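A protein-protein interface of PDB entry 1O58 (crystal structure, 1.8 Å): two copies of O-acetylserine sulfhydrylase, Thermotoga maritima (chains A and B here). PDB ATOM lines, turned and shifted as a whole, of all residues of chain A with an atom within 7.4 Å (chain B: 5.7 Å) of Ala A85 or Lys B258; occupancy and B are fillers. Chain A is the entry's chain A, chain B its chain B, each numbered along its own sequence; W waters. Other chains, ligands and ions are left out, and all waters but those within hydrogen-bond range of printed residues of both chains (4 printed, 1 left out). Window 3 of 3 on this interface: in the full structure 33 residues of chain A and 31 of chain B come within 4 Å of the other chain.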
ATOM      1  N   MET A  14      13.181   1.354 -15.009  1.00  0.00           N
ATOM      2  CA  MET A  14      14.457   2.060 -14.950  1.00  0.00           C
ATOM      3  C   MET A  14      14.285   3.397 -14.276  1.00  0.00           C
ATOM      4  O   MET A  14      15.187   3.841 -13.552  1.00  0.00           O
ATOM      5  CB  MET A  14      15.061   2.207 -16.353  1.00  0.00           C
ATOM      6  CG  MET A  14      15.519   0.863 -16.946  1.00  0.00           C
ATOM      7  SD  MET A  14      16.907   0.098 -16.016  1.00  0.00           S
ATOM      8  CE  MET A  14      16.796  -1.548 -16.752  1.00  0.00           C
ATOM      9  N   ALA A  79      24.982   1.839 -19.297  1.00  0.00           N
ATOM     10  CA  ALA A  79      23.710   2.427 -18.909  1.00  0.00           C
ATOM     11  C   ALA A  79      22.786   2.459 -20.122  1.00  0.00           C
ATOM     12  O   ALA A  79      21.653   2.050 -20.013  1.00  0.00           O
ATOM     13  CB  ALA A  79      23.902   3.812 -18.361  1.00  0.00           C
ATOM     14  N   ILE A  80      23.274   2.944 -21.265  1.00  0.00           N
ATOM     15  CA  ILE A  80      22.451   2.980 -22.478  1.00  0.00           C
ATOM     16  C   ILE A  80      22.043   1.593 -22.916  1.00  0.00           C
ATOM     17  O   ILE A  80      20.877   1.354 -23.270  1.00  0.00           O
ATOM     18  CB  ILE A  80      23.139   3.769 -23.630  1.00  0.00           C
ATOM     19  CG1 ILE A  80      23.279   5.236 -23.267  1.00  0.00           C
ATOM     20  CG2 ILE A  80      22.331   3.686 -24.903  1.00  0.00           C
ATOM     21  CD1 ILE A  80      24.290   5.994 -24.075  1.00  0.00           C
ATOM     22  N   ALA A  81      22.990   0.662 -22.868  1.00  0.00           N
ATOM     23  CA  ALA A  81      22.700  -0.711 -23.268  1.00  0.00           C
ATOM     24  C   ALA A  81      21.595  -1.336 -22.394  1.00  0.00           C
ATOM     25  O   ALA A  81      20.718  -2.065 -22.897  1.00  0.00           O
ATOM     26  CB  ALA A  81      23.965  -1.549 -23.206  1.00  0.00           C
ATOM     27  N   MET A  82      21.653  -1.087 -21.087  1.00  0.00           N
ATOM     28  CA  MET A  82      20.679  -1.618 -20.137  1.00  0.00           C
ATOM     29  C   MET A  82      19.294  -1.016 -20.406  1.00  0.00           C
ATOM     30  O   MET A  82      18.300  -1.722 -20.524  1.00  0.00           O
ATOM     31  CB  MET A  82      21.112  -1.243 -18.711  1.00  0.00           C
ATOM     32  CG  MET A  82      20.103  -1.516 -17.594  1.00  0.00           C
ATOM     33  SD  MET A  82      20.656  -0.972 -15.928  1.00  0.00           S
ATOM     34  CE  MET A  82      20.597   0.796 -16.192  1.00  0.00           C
ATOM     35  N   ILE A  83      19.243   0.301 -20.501  1.00  0.00           N
ATOM     36  CA  ILE A  83      17.954   0.990 -20.731  1.00  0.00           C
ATOM     37  C   ILE A  83      17.371   0.623 -22.089  1.00  0.00           C
ATOM     38  O   ILE A  83      16.179   0.377 -22.217  1.00  0.00           O
ATOM     39  CB  ILE A  83      18.114   2.508 -20.544  1.00  0.00           C
ATOM     40  CG1 ILE A  83      18.479   2.809 -19.087  1.00  0.00           C
ATOM     41  CG2 ILE A  83      16.801   3.229 -20.929  1.00  0.00           C
ATOM     42  CD1 ILE A  83      19.024   4.190 -18.854  1.00  0.00           C
ATOM     43  N   GLY A  84      18.216   0.500 -23.102  1.00  0.00           N
ATOM     44  CA  GLY A  84      17.781  -0.025 -24.406  1.00  0.00           C
ATOM     45  C   GLY A  84      17.282  -1.458 -24.436  1.00  0.00           C
ATOM     46  O   GLY A  84      16.342  -1.816 -25.177  1.00  0.00           O
ATOM     47  N   ALA A  85      17.932  -2.318 -23.677  1.00  0.00           N
ATOM     48  CA  ALA A  85      17.467  -3.692 -23.533  1.00  0.00           C
ATOM     49  C   ALA A  85      16.054  -3.757 -22.968  1.00  0.00           C
ATOM     50  O   ALA A  85      15.201  -4.486 -23.494  1.00  0.00           O
ATOM     51  CB  ALA A  85      18.395  -4.447 -22.649  1.00  0.00           C
ATOM     52  N   LYS A  86      15.814  -3.000 -21.903  1.00  0.00           N
ATOM     53  CA  LYS A  86      14.515  -2.977 -21.272  1.00  0.00           C
ATOM     54  C   LYS A  86      13.474  -2.283 -22.149  1.00  0.00           C
ATOM     55  O   LYS A  86      12.360  -2.800 -22.314  1.00  0.00           O
ATOM     56  CB  LYS A  86      14.584  -2.309 -19.883  1.00  0.00           C
ATOM     57  CG  LYS A  86      13.216  -2.170 -19.184  1.00  0.00           C
ATOM     58  CD  LYS A  86      12.462  -3.493 -19.070  1.00  0.00           C
ATOM     59  CE  LYS A  86      11.228  -3.363 -18.189  1.00  0.00           C
ATOM     60  NZ  LYS A  86      10.361  -4.607 -18.232  1.00  0.00           N
ATOM     61  N   ARG A  87      13.840  -1.137 -22.726  1.00  0.00           N
ATOM     62  CA  ARG A  87      12.869  -0.271 -23.417  1.00  0.00           C
ATOM     63  C   ARG A  87      12.711  -0.536 -24.914  1.00  0.00           C
ATOM     64  O   ARG A  87      11.859   0.063 -25.564  1.00  0.00           O
ATOM     65  CB  ARG A  87      13.195   1.227 -23.182  1.00  0.00           C
ATOM     66  CG  ARG A  87      13.159   1.662 -21.744  1.00  0.00           C
ATOM     67  CD  ARG A  87      13.497   3.151 -21.576  1.00  0.00           C
ATOM     68  NE  ARG A  87      12.403   4.033 -21.965  1.00  0.00           N
ATOM     69  CZ  ARG A  87      11.403   4.365 -21.155  1.00  0.00           C
ATOM     70  NH1 ARG A  87      11.301   3.814 -19.954  1.00  0.00           N
ATOM     71  NH2 ARG A  87      10.461   5.180 -21.574  1.00  0.00           N
ATOM     72  N   GLY A  88      13.528  -1.411 -25.486  1.00  0.00           N
ATOM     73  CA  GLY A  88      13.335  -1.811 -26.858  1.00  0.00           C
ATOM     74  C   GLY A  88      14.055  -1.006 -27.919  1.00  0.00           C
ATOM     75  O   GLY A  88      13.540  -0.885 -29.026  1.00  0.00           O
ATOM     76  N   HIS A  89      15.266  -0.540 -27.623  1.00  0.00           N
ATOM     77  CA  HIS A  89      16.077   0.230 -28.568  1.00  0.00           C
ATOM     78  C   HIS A  89      17.324  -0.576 -28.912  1.00  0.00           C
ATOM     79  O   HIS A  89      18.000  -1.115 -28.022  1.00  0.00           O
ATOM     80  CB  HIS A  89      16.553   1.542 -27.950  1.00  0.00           C
ATOM     81  CG  HIS A  89      15.447   2.439 -27.486  1.00  0.00           C
ATOM     82  ND1 HIS A  89      14.444   2.871 -28.334  1.00  0.00           N
ATOM     83  CD2 HIS A  89      15.214   3.023 -26.287  1.00  0.00           C
ATOM     84  CE1 HIS A  89      13.613   3.647 -27.655  1.00  0.00           C
ATOM     85  NE2 HIS A  89      14.056   3.760 -26.413  1.00  0.00           N
ATOM     86  N   ARG A  90      17.633  -0.646 -30.199  1.00  0.00           N
ATOM     87  CA  ARG A  90      18.920  -1.197 -30.623  1.00  0.00           C
ATOM     88  C   ARG A  90      20.017  -0.259 -30.129  1.00  0.00           C
ATOM     89  O   ARG A  90      19.897   0.963 -30.265  1.00  0.00           O
ATOM     90  CB  ARG A  90      18.983  -1.308 -32.131  1.00  0.00           C
ATOM     91  CG  ARG A  90      20.360  -1.778 -32.668  1.00  0.00           C
ATOM     92  CD  ARG A  90      20.567  -1.484 -34.108  1.00  0.00           C
ATOM     93  NE  ARG A  90      21.772  -2.130 -34.648  1.00  0.00           N
ATOM     94  CZ  ARG A  90      22.170  -2.016 -35.905  1.00  0.00           C
ATOM     95  NH1 ARG A  90      21.507  -1.249 -36.756  1.00  0.00           N
ATOM     96  NH2 ARG A  90      23.260  -2.654 -36.321  1.00  0.00           N
ATOM     97  N   VAL A  91      21.088  -0.820 -29.559  1.00  0.00           N
ATOM     98  CA  VAL A  91      22.204  -0.011 -29.047  1.00  0.00           C
ATOM     99  C   VAL A  91      23.524  -0.461 -29.659  1.00  0.00           C
ATOM    100  O   VAL A  91      23.861  -1.649 -29.577  1.00  0.00           O
ATOM    101  CB  VAL A  91      22.289  -0.093 -27.515  1.00  0.00           C
ATOM    102  CG1 VAL A  91      23.461   0.672 -27.002  1.00  0.00           C
ATOM    103  CG2 VAL A  91      20.994   0.474 -26.904  1.00  0.00           C
ATOM    104  N   LYS A 108      28.035  -7.098 -23.942  1.00  0.00           N
ATOM    105  CA  LYS A 108      27.552  -8.298 -24.600  1.00  0.00           C
ATOM    106  C   LYS A 108      26.369  -8.920 -23.864  1.00  0.00           C
ATOM    107  O   LYS A 108      25.373  -9.297 -24.485  1.00  0.00           O
ATOM    108  CB  LYS A 108      28.701  -9.307 -24.720  1.00  0.00           C
ATOM    109  CG  LYS A 108      28.327 -10.618 -25.356  1.00  0.00           C
ATOM    110  CD  LYS A 108      27.786 -10.409 -26.748  1.00  0.00           C
ATOM    111  CE  LYS A 108      27.852 -11.714 -27.560  1.00  0.00           C
ATOM    112  NZ  LYS A 108      26.831 -11.677 -28.662  1.00  0.00           N
ATOM    113  N   MET A 109      26.484  -9.051 -22.548  1.00  0.00           N
ATOM    114  CA  MET A 109      25.407  -9.571 -21.729  1.00  0.00           C
ATOM    115  C   MET A 109      24.093  -8.779 -21.931  1.00  0.00           C
ATOM    116  O   MET A 109      23.005  -9.358 -21.905  1.00  0.00           O
ATOM    117  CB  MET A 109      25.794  -9.537 -20.240  1.00  0.00           C
ATOM    118  CG  MET A 109      26.940 -10.500 -19.811  1.00  0.00           C
ATOM    119  SD  MET A 109      27.256 -10.316 -17.974  1.00  0.00           S
ATOM    120  CE  MET A 109      27.940  -9.127 -17.771  1.00  0.00           C
ATOM    121  N   LEU A 110      24.213  -7.474 -22.123  1.00  0.00           N
ATOM    122  CA  LEU A 110      23.040  -6.595 -22.304  1.00  0.00           C
ATOM    123  C   LEU A 110      22.544  -6.564 -23.740  1.00  0.00           C
ATOM    124  O   LEU A 110      21.551  -5.900 -24.052  1.00  0.00           O
ATOM    125  CB  LEU A 110      23.398  -5.195 -21.859  1.00  0.00           C
ATOM    126  CG  LEU A 110      23.629  -5.061 -20.356  1.00  0.00           C
ATOM    127  CD1 LEU A 110      24.261  -3.672 -20.088  1.00  0.00           C
ATOM    128  CD2 LEU A 110      22.348  -5.235 -19.556  1.00  0.00           C
ATOM    129  N   GLY A 111      23.238  -7.282 -24.615  1.00  0.00           N
ATOM    130  CA  GLY A 111      22.819  -7.415 -26.017  1.00  0.00           C
ATOM    131  C   GLY A 111      23.088  -6.190 -26.877  1.00  0.00           C
ATOM    132  O   GLY A 111      22.464  -6.006 -27.948  1.00  0.00           O
ATOM    133  N   ALA A 112      24.054  -5.380 -26.472  1.00  0.00           N
ATOM    134  CA  ALA A 112      24.483  -4.245 -27.281  1.00  0.00           C
ATOM    135  C   ALA A 112      25.546  -4.696 -28.286  1.00  0.00           C
ATOM    136  O   ALA A 112      26.185  -5.740 -28.124  1.00  0.00           O
ATOM    137  CB  ALA A 112      25.036  -3.139 -26.416  1.00  0.00           C
ATOM    138  N   ALA B 253      19.301 -16.412 -16.178  1.00  0.00           N
ATOM    139  CA  ALA B 253      20.211 -15.331 -15.854  1.00  0.00           C
ATOM    140  C   ALA B 253      20.594 -14.488 -17.091  1.00  0.00           C
ATOM    141  O   ALA B 253      20.510 -13.256 -17.073  1.00  0.00           O
ATOM    142  CB  ALA B 253      21.451 -15.840 -15.119  1.00  0.00           C
ATOM    143  N   ARG B 254      20.936 -15.151 -18.181  1.00  0.00           N
ATOM    144  CA  ARG B 254      21.271 -14.434 -19.420  1.00  0.00           C
ATOM    145  C   ARG B 254      20.034 -13.696 -19.931  1.00  0.00           C
ATOM    146  O   ARG B 254      20.107 -12.542 -20.406  1.00  0.00           O
ATOM    147  CB  ARG B 254      21.784 -15.405 -20.465  1.00  0.00           C
ATOM    148  CG  ARG B 254      23.113 -16.008 -20.068  1.00  0.00           C
ATOM    149  CD  ARG B 254      23.672 -16.935 -21.093  1.00  0.00           C
ATOM    150  NE  ARG B 254      24.787 -17.694 -20.549  1.00  0.00           N
ATOM    151  CZ  ARG B 254      24.847 -19.018 -20.473  1.00  0.00           C
ATOM    152  NH1 ARG B 254      23.848 -19.793 -20.887  1.00  0.00           N
ATOM    153  NH2 ARG B 254      25.942 -19.571 -19.976  1.00  0.00           N
ATOM    154  N   TYR B 255      18.880 -14.347 -19.803  1.00  0.00           N
ATOM    155  CA  TYR B 255      17.630 -13.771 -20.285  1.00  0.00           C
ATOM    156  C   TYR B 255      17.284 -12.500 -19.516  1.00  0.00           C
ATOM    157  O   TYR B 255      16.870 -11.482 -20.099  1.00  0.00           O
ATOM    158  CB  TYR B 255      16.513 -14.816 -20.174  1.00  0.00           C
ATOM    159  CG  TYR B 255      15.352 -14.570 -21.089  1.00  0.00           C
ATOM    160  CD1 TYR B 255      15.523 -14.560 -22.472  1.00  0.00           C
ATOM    161  CD2 TYR B 255      14.080 -14.324 -20.578  1.00  0.00           C
ATOM    162  CE1 TYR B 255      14.448 -14.343 -23.323  1.00  0.00           C
ATOM    163  CE2 TYR B 255      13.002 -14.091 -21.415  1.00  0.00           C
ATOM    164  CZ  TYR B 255      13.193 -14.094 -22.794  1.00  0.00           C
ATOM    165  OH  TYR B 255      12.114 -13.866 -23.636  1.00  0.00           O
ATOM    166  N   LEU B 256      17.503 -12.521 -18.207  1.00  0.00           N
ATOM    167  CA  LEU B 256      17.194 -11.353 -17.419  1.00  0.00           C
ATOM    168  C   LEU B 256      18.047 -10.153 -17.898  1.00  0.00           C
ATOM    169  O   LEU B 256      17.555  -9.038 -17.970  1.00  0.00           O
ATOM    170  CB  LEU B 256      17.424 -11.646 -15.932  1.00  0.00           C
ATOM    171  CG  LEU B 256      16.317 -12.502 -15.313  1.00  0.00           C
ATOM    172  CD1 LEU B 256      16.805 -13.249 -14.084  1.00  0.00           C
ATOM    173  CD2 LEU B 256      15.107 -11.634 -14.963  1.00  0.00           C
ATOM    174  N   ALA B 257      19.320 -10.400 -18.211  1.00  0.00           N
ATOM    175  CA  ALA B 257      20.201  -9.324 -18.669  1.00  0.00           C
ATOM    176  C   ALA B 257      19.734  -8.818 -20.029  1.00  0.00           C
ATOM    177  O   ALA B 257      19.619  -7.624 -20.245  1.00  0.00           O
ATOM    178  CB  ALA B 257      21.675  -9.772 -18.732  1.00  0.00           C
ATOM    179  N   LYS B 258      19.370  -9.730 -20.919  1.00  0.00           N
ATOM    180  CA  LYS B 258      19.052  -9.337 -22.304  1.00  0.00           C
ATOM    181  C   LYS B 258      17.661  -8.733 -22.435  1.00  0.00           C
ATOM    182  O   LYS B 258      17.462  -7.808 -23.222  1.00  0.00           O
ATOM    183  CB  LYS B 258      19.150 -10.538 -23.231  1.00  0.00           C
ATOM    184  CG  LYS B 258      20.584 -10.927 -23.568  1.00  0.00           C
ATOM    185  CD  LYS B 258      20.659 -12.215 -24.388  1.00  0.00           C
ATOM    186  CE  LYS B 258      21.773 -13.203 -23.850  1.00  0.00           C
ATOM    187  NZ  LYS B 258      21.832 -14.559 -24.476  1.00  0.00           N
ATOM    188  N   LYS B 259      16.697  -9.255 -21.680  1.00  0.00           N
ATOM    189  CA  LYS B 259      15.296  -8.794 -21.787  1.00  0.00           C
ATOM    190  C   LYS B 259      14.866  -7.741 -20.808  1.00  0.00           C
ATOM    191  O   LYS B 259      14.027  -6.897 -21.141  1.00  0.00           O
ATOM    192  CB  LYS B 259      14.332  -9.976 -21.697  1.00  0.00           C
ATOM    193  CG  LYS B 259      14.514 -10.916 -22.831  1.00  0.00           C
ATOM    194  CD  LYS B 259      13.750 -10.480 -24.086  1.00  0.00           C
ATOM    195  N   GLU B 260      15.429  -7.766 -19.606  1.00  0.00           N
ATOM    196  CA  GLU B 260      15.059  -6.809 -18.564  1.00  0.00           C
ATOM    197  C   GLU B 260      16.168  -5.805 -18.248  1.00  0.00           C
ATOM    198  O   GLU B 260      15.932  -4.846 -17.528  1.00  0.00           O
ATOM    199  CB  GLU B 260      14.644  -7.530 -17.273  1.00  0.00           C
ATOM    200  CG  GLU B 260      13.422  -8.429 -17.447  1.00  0.00           C
ATOM    201  CD  GLU B 260      12.100  -7.671 -17.468  1.00  0.00           C
ATOM    202  OE1 GLU B 260      11.054  -8.349 -17.614  1.00  0.00           O
ATOM    203  OE2 GLU B 260      12.108  -6.430 -17.338  1.00  0.00           O
ATOM    204  N   GLY B 261      17.367  -6.008 -18.781  1.00  0.00           N
ATOM    205  CA  GLY B 261      18.497  -5.117 -18.467  1.00  0.00           C
ATOM    206  C   GLY B 261      19.022  -5.312 -17.059  1.00  0.00           C
ATOM    207  O   GLY B 261      19.705  -4.437 -16.504  1.00  0.00           O
ATOM    208  N   LEU B 262      18.672  -6.440 -16.455  1.00  0.00           N
ATOM    209  CA  LEU B 262      19.015  -6.740 -15.074  1.00  0.00           C
ATOM    210  C   LEU B 262      20.274  -7.632 -14.957  1.00  0.00           C
ATOM    211  O   LEU B 262      20.263  -8.813 -15.320  1.00  0.00           O
ATOM    212  CB  LEU B 262      17.822  -7.400 -14.382  1.00  0.00           C
ATOM    213  CG  LEU B 262      16.592  -6.487 -14.210  1.00  0.00           C
ATOM    214  CD1 LEU B 262      15.392  -7.260 -13.654  1.00  0.00           C
ATOM    215  CD2 LEU B 262      16.947  -5.290 -13.344  1.00  0.00           C
HETATM  216  O   HOH W   1      19.272  -6.830 -25.189  1.00  0.00           O
HETATM  217  O   HOH W   2      20.980  -4.172 -14.029  1.00  0.00           O
HETATM  218  O   HOH W   3      22.701 -11.929 -21.423  1.00  0.00           O
HETATM  219  O   HOH W   4      15.627  -6.913 -25.079  1.00  0.00           O
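Of the printed residues of chain B, Met A82 touches Gly B261. Ile A83 touches none of the printed residues of chain B. Ala A85 touches just these residues of chain B: Lys B258 (3.5 Å) and Lys B259 (3.6 Å). Printed residues of chain B within 4 Å of Lys A86: Lys B259 (3.95 Å) and Glu B260 (2.7 Å). Ala A112 touches none of the printed residues of chain B. Of chain A, only Ala A85 (3.5 Å) and Met A109 (3.3 Å) come within 4 Å of Lys B258. Printed residues of chain A within 4 Å of Lys B259: Ala A85 (3.6 Å) and Lys A86 (3.95 Å). Of the printed residues of chain A, Glu B260 touches Met A14 (3.5 Å) and Lys A86 (2.7 Å). Of the printed residues of chain A, Gly B261 touches Met A82. The nearest residue of chain A that does not touch Lys B258 is Leu A110 (4.6 Å). The nearest printed residue of chain B that does not touch Leu A110 is Gly B261 (4.004 Å).
Among the printed residues, merely in contact across the chains: Met A109 with Lys B258 (3.3 Å), Met A109 with Ala B257 (3.5 Å), Met A14 with Glu B260 (3.5 Å), Ala A85 with Lys B258 (3.5 Å), Ala A85 with Lys B259 (3.6 Å), Leu A110 with Ala B257 (3.7 Å) and Lys A86 with Lys B259 (3.95 Å).
Water W3 bridges O of Met A109 and O of Arg B254. Water W1 lies within hydrogen-bond range of the backbone carbonyl oxygen (O) of Leu A110 (2.7 Å) and the backbone carbonyl oxygen (O) of Lys B258 (2.8 Å). Water W4 lies within hydrogen-bond range of O of Lys B258 and O of Ala A85. Water W2 lies within hydrogen-bond range of O of Gly B261 (2.8 Å) and SD of Met A82 (3.7 Å).
No position is printed for both chains.
The backbone carbonyl oxygen (O) of Leu B262 sits close to the backbone NH (N) of Ala B257. The backbone carbonyl oxygen (O) of Leu B256 is in hydrogen-bond range of the backbone NH (N) of Gly B261.
O of Gly B261 lies close to SD of Met A82 (3.6 Å). The side-chain amino group (NZ) of Lys A86 lies within salt-bridge range of the side-chain carboxylate (OE2) of Glu B260 (2.7 Å).
Of the 19 printed residues of chain A, 6 touch a printed residue of chain B. Printed residues of chain A that touch a printed residue of chain B: Met A14, Met A82, Ala A85, Lys A86, Met A109 and Leu A110. Printed residues of chain B that touch a printed residue of chain A: Ala B257, Lys B258, Lys B259, Glu B260 and Gly B261. Hydrophobic or aromatic side chains of chain B that line the printed part of chain A: Ala B257. Among the printed residues, Asp or Glu carboxylates within 4 Å of a Lys or Arg side-chain nitrogen of the other chain: Lys A86 with Glu B260 (2.7 Å).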
